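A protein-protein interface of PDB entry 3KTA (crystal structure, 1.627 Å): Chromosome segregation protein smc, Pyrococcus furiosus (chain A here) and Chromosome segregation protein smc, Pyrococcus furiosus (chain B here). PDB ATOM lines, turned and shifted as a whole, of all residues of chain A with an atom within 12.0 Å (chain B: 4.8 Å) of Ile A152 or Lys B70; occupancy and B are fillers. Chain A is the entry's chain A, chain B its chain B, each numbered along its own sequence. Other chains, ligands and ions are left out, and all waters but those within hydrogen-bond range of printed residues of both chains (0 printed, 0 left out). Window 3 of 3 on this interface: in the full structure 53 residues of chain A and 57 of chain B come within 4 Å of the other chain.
Of the printed residues of chain B, Ile A152 touches Lys B70 (3.8 Å) and Thr B73 (3.8 Å).
Lys B70 touches just these residues of chain A: Thr A149 and Ile A152.
Ile B50 touches one residue of chain A.
No residue of chain A comes within 4 Å of Ile B62.
No residue of chain A comes within 4 Å of Glu B63.
Met B65 touches none of the printed residues of chain A.
No residue of chain A comes within 4 Å of Ser B66.
No residue of chain A comes within 4 Å of Gly B67.
No residue of chain A comes within 4 Å of Gly B68.
No residue of chain A comes within 4 Å of Leu B72.
Thr B73 touches just one residue of chain A: Ile A152.
Of the printed residues of chain B, Arg A159 touches Ile B50 (3.6 Å).
Of the printed residues of chain A, Ala B74 touches Ile A148 and Phe A151.
Of the printed residues of chain B, Thr A149 touches Lys B70.
Printed residues of chain B within 4 Å of Ile A148: Ala B74.
Of the printed residues of chain B, Phe A151 touches Ala B74.
Glu A158 touches none of the printed residues of chain B.
The nearest printed residue of chain B that does not touch Ile A152 is Ala B74 (4.01 Å).
The nearest residue of chain A that does not touch Lys B70 is Ile A148 (5.6 Å).
The nearest printed residue of chain A that does not touch Ala B74 is Ile A152 (4.01 Å).
Of the 20 printed residues of chain A, 5 touch a printed residue of chain B.
Printed residues of chain A that touch a printed residue of chain B: Ile A148, Thr A149, Phe A151, Ile A152 and Arg A159.
Hydrophobic or aromatic side chains of chain A within 4 Å of the printed part of chain B: Ile A148, Phe A151 and Ile A152.
Of the 13 printed residues of chain B, 4 touch a printed residue of chain A.
Along chain B the printed residues that touch a printed residue of chain A span positions 50 to 74.
The backbone carbonyl oxygen of Phe A151 is in hydrogen-bond range of the guanidinium group of Arg A159 (2.9 Å).
The backbone carbonyl oxygen of Met A154 sits at hydrogen-bond distance from the guanidinium group of Arg A159 (3.2 Å).
O of Ile B62 is in hydrogen-bond range of NZ of Lys B70.
SD of Met B65 lies close to OG1 of Thr B73 (3.6 Å).
O of Glu B69 is in hydrogen-bond range of OG1 of Thr B73 (2.8 Å).
Ile A148 touches Ala B74.
Thr A149 touches Lys B70.
Phe A151 touches Ala B74 (CB to CB, 3.9997 Å).
Ile A152 touches Lys B70 (CD1 to CG, 3.8 Å).
Ile A152 touches Thr B73 (CG2 to CG2, 3.8 Å).
CD1 of Ile B50 touches NE of Arg A159, at 3.6 Å.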
ATOM      1  N   TYR A 140      -0.966  20.804  -0.121  1.00  0.00           N
ATOM      2  CA  TYR A 140      -1.455  20.684  -1.497  1.00  0.00           C
ATOM      3  C   TYR A 140      -0.654  19.608  -2.242  1.00  0.00           C
ATOM      4  O   TYR A 140      -1.066  19.131  -3.297  1.00  0.00           O
ATOM      5  CB  TYR A 140      -1.309  22.009  -2.263  1.00  0.00           C
ATOM      6  CG  TYR A 140       0.106  22.230  -2.789  1.00  0.00           C
ATOM      7  CD1 TYR A 140       1.105  22.689  -1.947  1.00  0.00           C
ATOM      8  CD2 TYR A 140       0.435  21.959  -4.116  1.00  0.00           C
ATOM      9  CE1 TYR A 140       2.399  22.872  -2.409  1.00  0.00           C
ATOM     10  CE2 TYR A 140       1.727  22.137  -4.587  1.00  0.00           C
ATOM     11  CZ  TYR A 140       2.702  22.596  -3.725  1.00  0.00           C
ATOM     12  OH  TYR A 140       3.992  22.774  -4.164  1.00  0.00           O
ATOM     13  N   ILE A 142       0.121  16.668  -1.260  1.00  0.00           N
ATOM     14  CA  ILE A 142      -0.347  15.307  -1.017  1.00  0.00           C
ATOM     15  C   ILE A 142      -1.721  15.176  -1.659  1.00  0.00           C
ATOM     16  O   ILE A 142      -2.658  15.870  -1.284  1.00  0.00           O
ATOM     17  CB  ILE A 142      -0.328  14.958   0.494  1.00  0.00           C
ATOM     18  CG1 ILE A 142       1.131  14.823   0.982  1.00  0.00           C
ATOM     19  CG2 ILE A 142      -1.105  13.671   0.771  1.00  0.00           C
ATOM     20  CD1 ILE A 142       1.268  14.554   2.474  1.00  0.00           C
ATOM     21  N   VAL A 143      -1.832  14.333  -2.683  1.00  0.00           N
ATOM     22  CA  VAL A 143      -3.100  14.188  -3.390  1.00  0.00           C
ATOM     23  C   VAL A 143      -3.612  12.764  -3.245  1.00  0.00           C
ATOM     24  O   VAL A 143      -3.132  11.838  -3.920  1.00  0.00           O
ATOM     25  CB  VAL A 143      -2.976  14.551  -4.889  1.00  0.00           C
ATOM     26  CG1 VAL A 143      -4.345  14.467  -5.570  1.00  0.00           C
ATOM     27  CG2 VAL A 143      -2.355  15.955  -5.064  1.00  0.00           C
ATOM     28  N   LEU A 144      -4.572  12.578  -2.342  1.00  0.00           N
ATOM     29  CA  LEU A 144      -5.062  11.243  -2.006  1.00  0.00           C
ATOM     30  C   LEU A 144      -5.958  10.707  -3.116  1.00  0.00           C
ATOM     31  O   LEU A 144      -6.386  11.456  -4.005  1.00  0.00           O
ATOM     32  CB  LEU A 144      -5.805  11.260  -0.665  1.00  0.00           C
ATOM     33  CG  LEU A 144      -4.992  11.816   0.515  1.00  0.00           C
ATOM     34  CD1 LEU A 144      -5.878  11.932   1.739  1.00  0.00           C
ATOM     35  CD2 LEU A 144      -3.755  10.956   0.786  1.00  0.00           C
ATOM     36  N   GLY A 146      -8.639   9.783  -5.601  1.00  0.00           N
ATOM     37  CA  GLY A 146      -9.892  10.423  -5.952  1.00  0.00           C
ATOM     38  C   GLY A 146      -9.984  11.912  -5.656  1.00  0.00           C
ATOM     39  O   GLY A 146     -11.051  12.505  -5.830  1.00  0.00           O
ATOM     40  N   ASP A 147      -8.875  12.527  -5.248  1.00  0.00           N
ATOM     41  CA  ASP A 147      -8.923  13.892  -4.740  1.00  0.00           C
ATOM     42  C   ASP A 147      -8.161  14.913  -5.597  1.00  0.00           C
ATOM     43  O   ASP A 147      -7.984  16.057  -5.181  1.00  0.00           O
ATOM     44  CB  ASP A 147      -8.395  13.920  -3.298  1.00  0.00           C
ATOM     45  CG  ASP A 147      -9.055  14.989  -2.448  1.00  0.00           C
ATOM     46  OD1 ASP A 147     -10.176  15.425  -2.786  1.00  0.00           O
ATOM     47  OD2 ASP A 147      -8.451  15.389  -1.428  1.00  0.00           O
ATOM     48  N   ILE A 148      -7.705  14.526  -6.789  1.00  0.00           N
ATOM     49  CA  ILE A 148      -6.938  15.487  -7.593  1.00  0.00           C
ATOM     50  C   ILE A 148      -7.735  16.749  -7.906  1.00  0.00           C
ATOM     51  O   ILE A 148      -7.172  17.840  -7.988  1.00  0.00           O
ATOM     52  CB  ILE A 148      -6.365  14.897  -8.902  1.00  0.00           C
ATOM     53  CG1 ILE A 148      -5.553  15.966  -9.643  1.00  0.00           C
ATOM     54  CG2 ILE A 148      -7.471  14.381  -9.783  1.00  0.00           C
ATOM     55  CD1 ILE A 148      -4.299  16.461  -8.902  1.00  0.00           C
ATOM     56  N   THR A 149      -9.045  16.614  -8.057  1.00  0.00           N
ATOM     57  CA  THR A 149      -9.852  17.767  -8.411  1.00  0.00           C
ATOM     58  C   THR A 149     -10.205  18.643  -7.215  1.00  0.00           C
ATOM     59  O   THR A 149     -10.949  19.604  -7.362  1.00  0.00           O
ATOM     60  CB  THR A 149     -11.141  17.374  -9.165  1.00  0.00           C
ATOM     61  OG1 THR A 149     -11.938  16.517  -8.342  1.00  0.00           O
ATOM     62  CG2 THR A 149     -10.799  16.666 -10.480  1.00  0.00           C
ATOM     63  N   LYS A 150      -9.663  18.336  -6.036  1.00  0.00           N
ATOM     64  CA  LYS A 150      -9.828  19.252  -4.900  1.00  0.00           C
ATOM     65  C   LYS A 150      -9.450  20.682  -5.304  1.00  0.00           C
ATOM     66  O   LYS A 150     -10.028  21.653  -4.816  1.00  0.00           O
ATOM     67  CB  LYS A 150      -9.003  18.821  -3.678  1.00  0.00           C
ATOM     68  CG  LYS A 150      -7.487  18.836  -3.871  1.00  0.00           C
ATOM     69  CD  LYS A 150      -6.758  18.412  -2.580  1.00  0.00           C
ATOM     70  CE  LYS A 150      -5.309  17.992  -2.868  1.00  0.00           C
ATOM     71  NZ  LYS A 150      -4.472  17.811  -1.642  1.00  0.00           N
ATOM     72  N   PHE A 151      -8.477  20.802  -6.199  1.00  0.00           N
ATOM     73  CA  PHE A 151      -7.987  22.102  -6.632  1.00  0.00           C
ATOM     74  C   PHE A 151      -8.986  22.825  -7.523  1.00  0.00           C
ATOM     75  O   PHE A 151      -8.967  24.050  -7.623  1.00  0.00           O
ATOM     76  CB  PHE A 151      -6.641  21.954  -7.333  1.00  0.00           C
ATOM     77  CG  PHE A 151      -5.567  21.405  -6.444  1.00  0.00           C
ATOM     78  CD1 PHE A 151      -4.968  22.208  -5.485  1.00  0.00           C
ATOM     79  CD2 PHE A 151      -5.171  20.079  -6.549  1.00  0.00           C
ATOM     80  CE1 PHE A 151      -3.981  21.699  -4.651  1.00  0.00           C
ATOM     81  CE2 PHE A 151      -4.188  19.569  -5.722  1.00  0.00           C
ATOM     82  CZ  PHE A 151      -3.588  20.376  -4.778  1.00  0.00           C
ATOM     83  N   ILE A 152      -9.859  22.075  -8.184  1.00  0.00           N
ATOM     84  CA  ILE A 152     -10.878  22.741  -8.991  1.00  0.00           C
ATOM     85  C   ILE A 152     -12.214  22.842  -8.238  1.00  0.00           C
ATOM     86  O   ILE A 152     -13.079  23.632  -8.618  1.00  0.00           O
ATOM     87  CB  ILE A 152     -11.000  22.157 -10.434  1.00  0.00           C
ATOM     88  CG1 ILE A 152     -11.260  20.659 -10.417  1.00  0.00           C
ATOM     89  CG2 ILE A 152      -9.730  22.445 -11.241  1.00  0.00           C
ATOM     90  CD1 ILE A 152     -12.720  20.280 -10.265  1.00  0.00           C
ATOM     91  N   LYS A 153     -12.356  22.080  -7.151  1.00  0.00           N
ATOM     92  CA  LYS A 153     -13.566  22.117  -6.322  1.00  0.00           C
ATOM     93  C   LYS A 153     -13.524  23.211  -5.252  1.00  0.00           C
ATOM     94  O   LYS A 153     -14.574  23.675  -4.795  1.00  0.00           O
ATOM     95  CB  LYS A 153     -13.828  20.752  -5.664  1.00  0.00           C
ATOM     96  CG  LYS A 153     -14.006  19.608  -6.667  1.00  0.00           C
ATOM     97  CD  LYS A 153     -14.464  18.310  -5.999  1.00  0.00           C
ATOM     98  CE  LYS A 153     -13.444  17.785  -5.004  1.00  0.00           C
ATOM     99  N   MET A 154     -12.318  23.611  -4.852  1.00  0.00           N
ATOM    100  CA  MET A 154     -12.145  24.638  -3.817  1.00  0.00           C
ATOM    101  C   MET A 154     -12.674  26.001  -4.267  1.00  0.00           C
ATOM    102  O   MET A 154     -12.719  26.294  -5.463  1.00  0.00           O
ATOM    103  CB  MET A 154     -10.678  24.736  -3.357  1.00  0.00           C
ATOM    104  CG  MET A 154      -9.658  25.089  -4.451  1.00  0.00           C
ATOM    105  SD  MET A 154      -7.805  25.218  -3.790  1.00  0.00           S
ATOM    106  CE  MET A 154      -7.689  23.482  -2.903  1.00  0.00           C
ATOM    107  N   SER A 155     -13.090  26.826  -3.310  1.00  0.00           N
ATOM    108  CA  SER A 155     -13.583  28.163  -3.644  1.00  0.00           C
ATOM    109  C   SER A 155     -12.433  29.012  -4.148  1.00  0.00           C
ATOM    110  O   SER A 155     -11.285  28.784  -3.761  1.00  0.00           O
ATOM    111  CB  SER A 155     -14.193  28.850  -2.420  1.00  0.00           C
ATOM    112  OG  SER A 155     -13.181  29.238  -1.507  1.00  0.00           O
ATOM    113  N   PRO A 156     -12.733  30.006  -5.001  1.00  0.00           N
ATOM    114  CA  PRO A 156     -11.706  30.972  -5.394  1.00  0.00           C
ATOM    115  C   PRO A 156     -10.963  31.526  -4.187  1.00  0.00           C
ATOM    116  O   PRO A 156      -9.757  31.746  -4.246  1.00  0.00           O
ATOM    117  CB  PRO A 156     -12.520  32.069  -6.075  1.00  0.00           C
ATOM    118  CG  PRO A 156     -13.656  31.322  -6.703  1.00  0.00           C
ATOM    119  CD  PRO A 156     -14.007  30.247  -5.705  1.00  0.00           C
ATOM    120  N   LEU A 157     -11.671  31.735  -3.083  1.00  0.00           N
ATOM    121  CA  LEU A 157     -11.020  32.278  -1.896  1.00  0.00           C
ATOM    122  C   LEU A 157     -10.000  31.298  -1.306  1.00  0.00           C
ATOM    123  O   LEU A 157      -8.877  31.692  -1.000  1.00  0.00           O
ATOM    124  CB  LEU A 157     -12.057  32.699  -0.849  1.00  0.00           C
ATOM    125  CG  LEU A 157     -11.597  33.615   0.283  1.00  0.00           C
ATOM    126  CD1 LEU A 157     -10.728  34.764  -0.212  1.00  0.00           C
ATOM    127  CD2 LEU A 157     -12.821  34.163   1.000  1.00  0.00           C
ATOM    128  N   GLU A 158     -10.382  30.029  -1.149  1.00  0.00           N
ATOM    129  CA  GLU A 158      -9.437  29.021  -0.675  1.00  0.00           C
ATOM    130  C   GLU A 158      -8.240  28.940  -1.614  1.00  0.00           C
ATOM    131  O   GLU A 158      -7.100  28.761  -1.179  1.00  0.00           O
ATOM    132  CB  GLU A 158     -10.091  27.638  -0.540  1.00  0.00           C
ATOM    133  CG  GLU A 158      -9.071  26.536  -0.232  1.00  0.00           C
ATOM    134  CD  GLU A 158      -9.693  25.244   0.258  1.00  0.00           C
ATOM    135  OE1 GLU A 158      -8.929  24.288   0.504  1.00  0.00           O
ATOM    136  OE2 GLU A 158     -10.930  25.185   0.410  1.00  0.00           O
ATOM    137  N   ARG A 159      -8.497  29.084  -2.905  1.00  0.00           N
ATOM    138  CA  ARG A 159      -7.408  28.969  -3.871  1.00  0.00           C
ATOM    139  C   ARG A 159      -6.389  30.102  -3.703  1.00  0.00           C
ATOM    140  O   ARG A 159      -5.179  29.872  -3.764  1.00  0.00           O
ATOM    141  CB  ARG A 159      -7.949  28.887  -5.296  1.00  0.00           C
ATOM    142  CG  ARG A 159      -6.887  28.525  -6.332  1.00  0.00           C
ATOM    143  CD  ARG A 159      -7.497  28.322  -7.720  1.00  0.00           C
ATOM    144  NE  ARG A 159      -8.488  27.253  -7.746  1.00  0.00           N
ATOM    145  CZ  ARG A 159      -9.796  27.441  -7.893  1.00  0.00           C
ATOM    146  NH1 ARG A 159     -10.286  28.665  -8.035  1.00  0.00           N
ATOM    147  NH2 ARG A 159     -10.619  26.402  -7.907  1.00  0.00           N
ATOM    148  N   ARG A 160      -6.859  31.320  -3.433  1.00  0.00           N
ATOM    149  CA  ARG A 160      -5.916  32.407  -3.250  1.00  0.00           C
ATOM    150  C   ARG A 160      -5.095  32.220  -1.987  1.00  0.00           C
ATOM    151  O   ARG A 160      -3.911  32.543  -1.937  1.00  0.00           O
ATOM    152  CB  ARG A 160      -6.614  33.768  -3.233  1.00  0.00           C
ATOM    153  CG  ARG A 160      -5.641  34.925  -3.455  1.00  0.00           C
ATOM    154  CD  ARG A 160      -6.007  36.131  -2.592  1.00  0.00           C
ATOM    155  NE  ARG A 160      -5.670  35.910  -1.191  1.00  0.00           N
ATOM    156  CZ  ARG A 160      -6.540  35.996  -0.186  1.00  0.00           C
ATOM    157  NH1 ARG A 160      -7.804  36.309  -0.426  1.00  0.00           N
ATOM    158  NH2 ARG A 160      -6.139  35.790   1.058  1.00  0.00           N
ATOM    159  N   LEU A 162      -4.033  29.535  -0.706  1.00  0.00           N
ATOM    160  CA  LEU A 162      -2.928  28.637  -1.026  1.00  0.00           C
ATOM    161  C   LEU A 162      -1.739  29.429  -1.573  1.00  0.00           C
ATOM    162  O   LEU A 162      -0.596  29.217  -1.165  1.00  0.00           O
ATOM    163  CB  LEU A 162      -3.384  27.555  -2.009  1.00  0.00           C
ATOM    164  CG  LEU A 162      -2.345  26.514  -2.431  1.00  0.00           C
ATOM    165  CD1 LEU A 162      -1.665  25.896  -1.218  1.00  0.00           C
ATOM    166  CD2 LEU A 162      -2.996  25.439  -3.291  1.00  0.00           C
ATOM    167  N   ILE B  50      -9.920  30.183 -11.965  1.00  0.00           N
ATOM    168  CA  ILE B  50      -9.303  29.523 -13.107  1.00  0.00           C
ATOM    169  C   ILE B  50     -10.241  29.670 -14.285  1.00  0.00           C
ATOM    170  O   ILE B  50     -11.438  29.422 -14.159  1.00  0.00           O
ATOM    171  CB  ILE B  50      -9.079  28.020 -12.828  1.00  0.00           C
ATOM    172  CG1 ILE B  50      -8.082  27.842 -11.685  1.00  0.00           C
ATOM    173  CG2 ILE B  50      -8.592  27.301 -14.090  1.00  0.00           C
ATOM    174  CD1 ILE B  50      -7.896  26.407 -11.239  1.00  0.00           C
ATOM    175  N   ILE B  62     -15.867  25.228 -15.314  1.00  0.00           N
ATOM    176  CA  ILE B  62     -15.402  24.059 -14.571  1.00  0.00           C
ATOM    177  C   ILE B  62     -16.491  23.002 -14.431  1.00  0.00           C
ATOM    178  O   ILE B  62     -16.240  21.813 -14.627  1.00  0.00           O
ATOM    179  CB  ILE B  62     -14.911  24.455 -13.165  1.00  0.00           C
ATOM    180  CG1 ILE B  62     -13.690  25.372 -13.260  1.00  0.00           C
ATOM    181  CG2 ILE B  62     -14.575  23.222 -12.342  1.00  0.00           C
ATOM    182  CD1 ILE B  62     -12.500  24.732 -13.925  1.00  0.00           C
ATOM    183  N   GLU B  63     -17.702  23.445 -14.098  1.00  0.00           N
ATOM    184  CA  GLU B  63     -18.839  22.542 -13.902  1.00  0.00           C
ATOM    185  C   GLU B  63     -19.176  21.736 -15.157  1.00  0.00           C
ATOM    186  O   GLU B  63     -19.758  20.649 -15.075  1.00  0.00           O
ATOM    187  CB  GLU B  63     -20.075  23.332 -13.441  1.00  0.00           C
ATOM    188  CG  GLU B  63     -19.883  24.125 -12.163  1.00  0.00           C
ATOM    189  CD  GLU B  63     -19.356  25.527 -12.402  1.00  0.00           C
ATOM    190  OE1 GLU B  63     -19.152  25.904 -13.575  1.00  0.00           O
ATOM    191  OE2 GLU B  63     -19.151  26.258 -11.410  1.00  0.00           O
ATOM    192  N   MET B  65     -16.835  20.749 -17.299  1.00  0.00           N
ATOM    193  CA  MET B  65     -15.663  19.971 -17.675  1.00  0.00           C
ATOM    194  C   MET B  65     -15.868  18.489 -17.410  1.00  0.00           C
ATOM    195  O   MET B  65     -16.551  18.110 -16.467  1.00  0.00           O
ATOM    196  CB  MET B  65     -14.446  20.433 -16.884  1.00  0.00           C
ATOM    197  CG  MET B  65     -13.789  21.663 -17.430  1.00  0.00           C
ATOM    198  SD  MET B  65     -12.183  22.003 -16.368  1.00  0.00           S
ATOM    199  CE  MET B  65     -11.568  23.587 -17.315  1.00  0.00           C
ATOM    200  N   SER B  66     -15.239  17.666 -18.241  1.00  0.00           N
ATOM    201  CA  SER B  66     -15.156  16.235 -18.018  1.00  0.00           C
ATOM    202  C   SER B  66     -14.208  15.939 -16.865  1.00  0.00           C
ATOM    203  O   SER B  66     -13.461  16.814 -16.425  1.00  0.00           O
ATOM    204  CB  SER B  66     -14.608  15.556 -19.266  1.00  0.00           C
ATOM    205  OG  SER B  66     -13.235  15.877 -19.451  1.00  0.00           O
ATOM    206  N   GLY B  67     -14.225  14.696 -16.390  1.00  0.00           N
ATOM    207  CA  GLY B  67     -13.333  14.292 -15.322  1.00  0.00           C
ATOM    208  C   GLY B  67     -11.891  14.521 -15.728  1.00  0.00           C
ATOM    209  O   GLY B  67     -11.081  15.012 -14.936  1.00  0.00           O
ATOM    210  N   GLY B  68     -11.572  14.161 -16.966  1.00  0.00           N
ATOM    211  CA  GLY B  68     -10.228  14.334 -17.491  1.00  0.00           C
ATOM    212  C   GLY B  68      -9.820  15.796 -17.558  1.00  0.00           C
ATOM    213  O   GLY B  68      -8.704  16.159 -17.192  1.00  0.00           O
ATOM    214  N   GLU B  69     -10.725  16.638 -18.038  1.00  0.00           N
ATOM    215  CA  GLU B  69     -10.456  18.070 -18.110  1.00  0.00           C
ATOM    216  C   GLU B  69     -10.200  18.660 -16.722  1.00  0.00           C
ATOM    217  O   GLU B  69      -9.272  19.461 -16.539  1.00  0.00           O
ATOM    218  CB  GLU B  69     -11.609  18.792 -18.819  1.00  0.00           C
ATOM    219  CG  GLU B  69     -11.624  18.509 -20.314  1.00  0.00           C
ATOM    220  CD  GLU B  69     -12.861  19.024 -21.016  1.00  0.00           C
ATOM    221  OE1 GLU B  69     -13.901  19.210 -20.350  1.00  0.00           O
ATOM    222  OE2 GLU B  69     -12.782  19.239 -22.243  1.00  0.00           O
ATOM    223  N   LYS B  70     -11.010  18.267 -15.743  1.00  0.00           N
ATOM    224  CA  LYS B  70     -10.807  18.727 -14.368  1.00  0.00           C
ATOM    225  C   LYS B  70      -9.440  18.317 -13.819  1.00  0.00           C
ATOM    226  O   LYS B  70      -8.746  19.135 -13.168  1.00  0.00           O
ATOM    227  CB  LYS B  70     -11.912  18.196 -13.448  1.00  0.00           C
ATOM    228  CG  LYS B  70     -13.275  18.814 -13.699  1.00  0.00           C
ATOM    229  CD  LYS B  70     -14.332  18.062 -12.900  1.00  0.00           C
ATOM    230  CE  LYS B  70     -15.740  18.529 -13.227  1.00  0.00           C
ATOM    231  NZ  LYS B  70     -15.925  19.900 -12.712  1.00  0.00           N
ATOM    232  N   ALA B  71      -9.046  17.070 -14.088  1.00  0.00           N
ATOM    233  CA  ALA B  71      -7.776  16.533 -13.591  1.00  0.00           C
ATOM    234  C   ALA B  71      -6.620  17.289 -14.202  1.00  0.00           C
ATOM    235  O   ALA B  71      -5.696  17.679 -13.501  1.00  0.00           O
ATOM    236  CB  ALA B  71      -7.651  15.046 -13.901  1.00  0.00           C
ATOM    237  N   LEU B  72      -6.680  17.515 -15.507  1.00  0.00           N
ATOM    238  CA  LEU B  72      -5.599  18.234 -16.179  1.00  0.00           C
ATOM    239  C   LEU B  72      -5.471  19.665 -15.693  1.00  0.00           C
ATOM    240  O   LEU B  72      -4.372  20.182 -15.536  1.00  0.00           O
ATOM    241  CB  LEU B  72      -5.779  18.220 -17.688  1.00  0.00           C
ATOM    242  CG  LEU B  72      -5.488  16.870 -18.328  1.00  0.00           C
ATOM    243  CD1 LEU B  72      -5.712  16.932 -19.836  1.00  0.00           C
ATOM    244  CD2 LEU B  72      -4.069  16.399 -18.003  1.00  0.00           C
ATOM    245  N   THR B  73      -6.606  20.304 -15.443  1.00  0.00           N
ATOM    246  CA  THR B  73      -6.601  21.667 -14.949  1.00  0.00           C
ATOM    247  C   THR B  73      -5.965  21.730 -13.553  1.00  0.00           C
ATOM    248  O   THR B  73      -5.127  22.595 -13.277  1.00  0.00           O
ATOM    249  CB  THR B  73      -8.041  22.233 -14.924  1.00  0.00           C
ATOM    250  OG1 THR B  73      -8.569  22.201 -16.257  1.00  0.00           O
ATOM    251  CG2 THR B  73      -8.041  23.663 -14.436  1.00  0.00           C
ATOM    252  N   ALA B  74      -6.373  20.803 -12.685  1.00  0.00           N
ATOM    253  CA  ALA B  74      -5.839  20.682 -11.328  1.00  0.00           C
ATOM    254  C   ALA B  74      -4.346  20.374 -11.359  1.00  0.00           C
ATOM    255  O   ALA B  74      -3.580  20.938 -10.580  1.00  0.00           O
ATOM    256  CB  ALA B  74      -6.575  19.596 -10.563  1.00  0.00           C
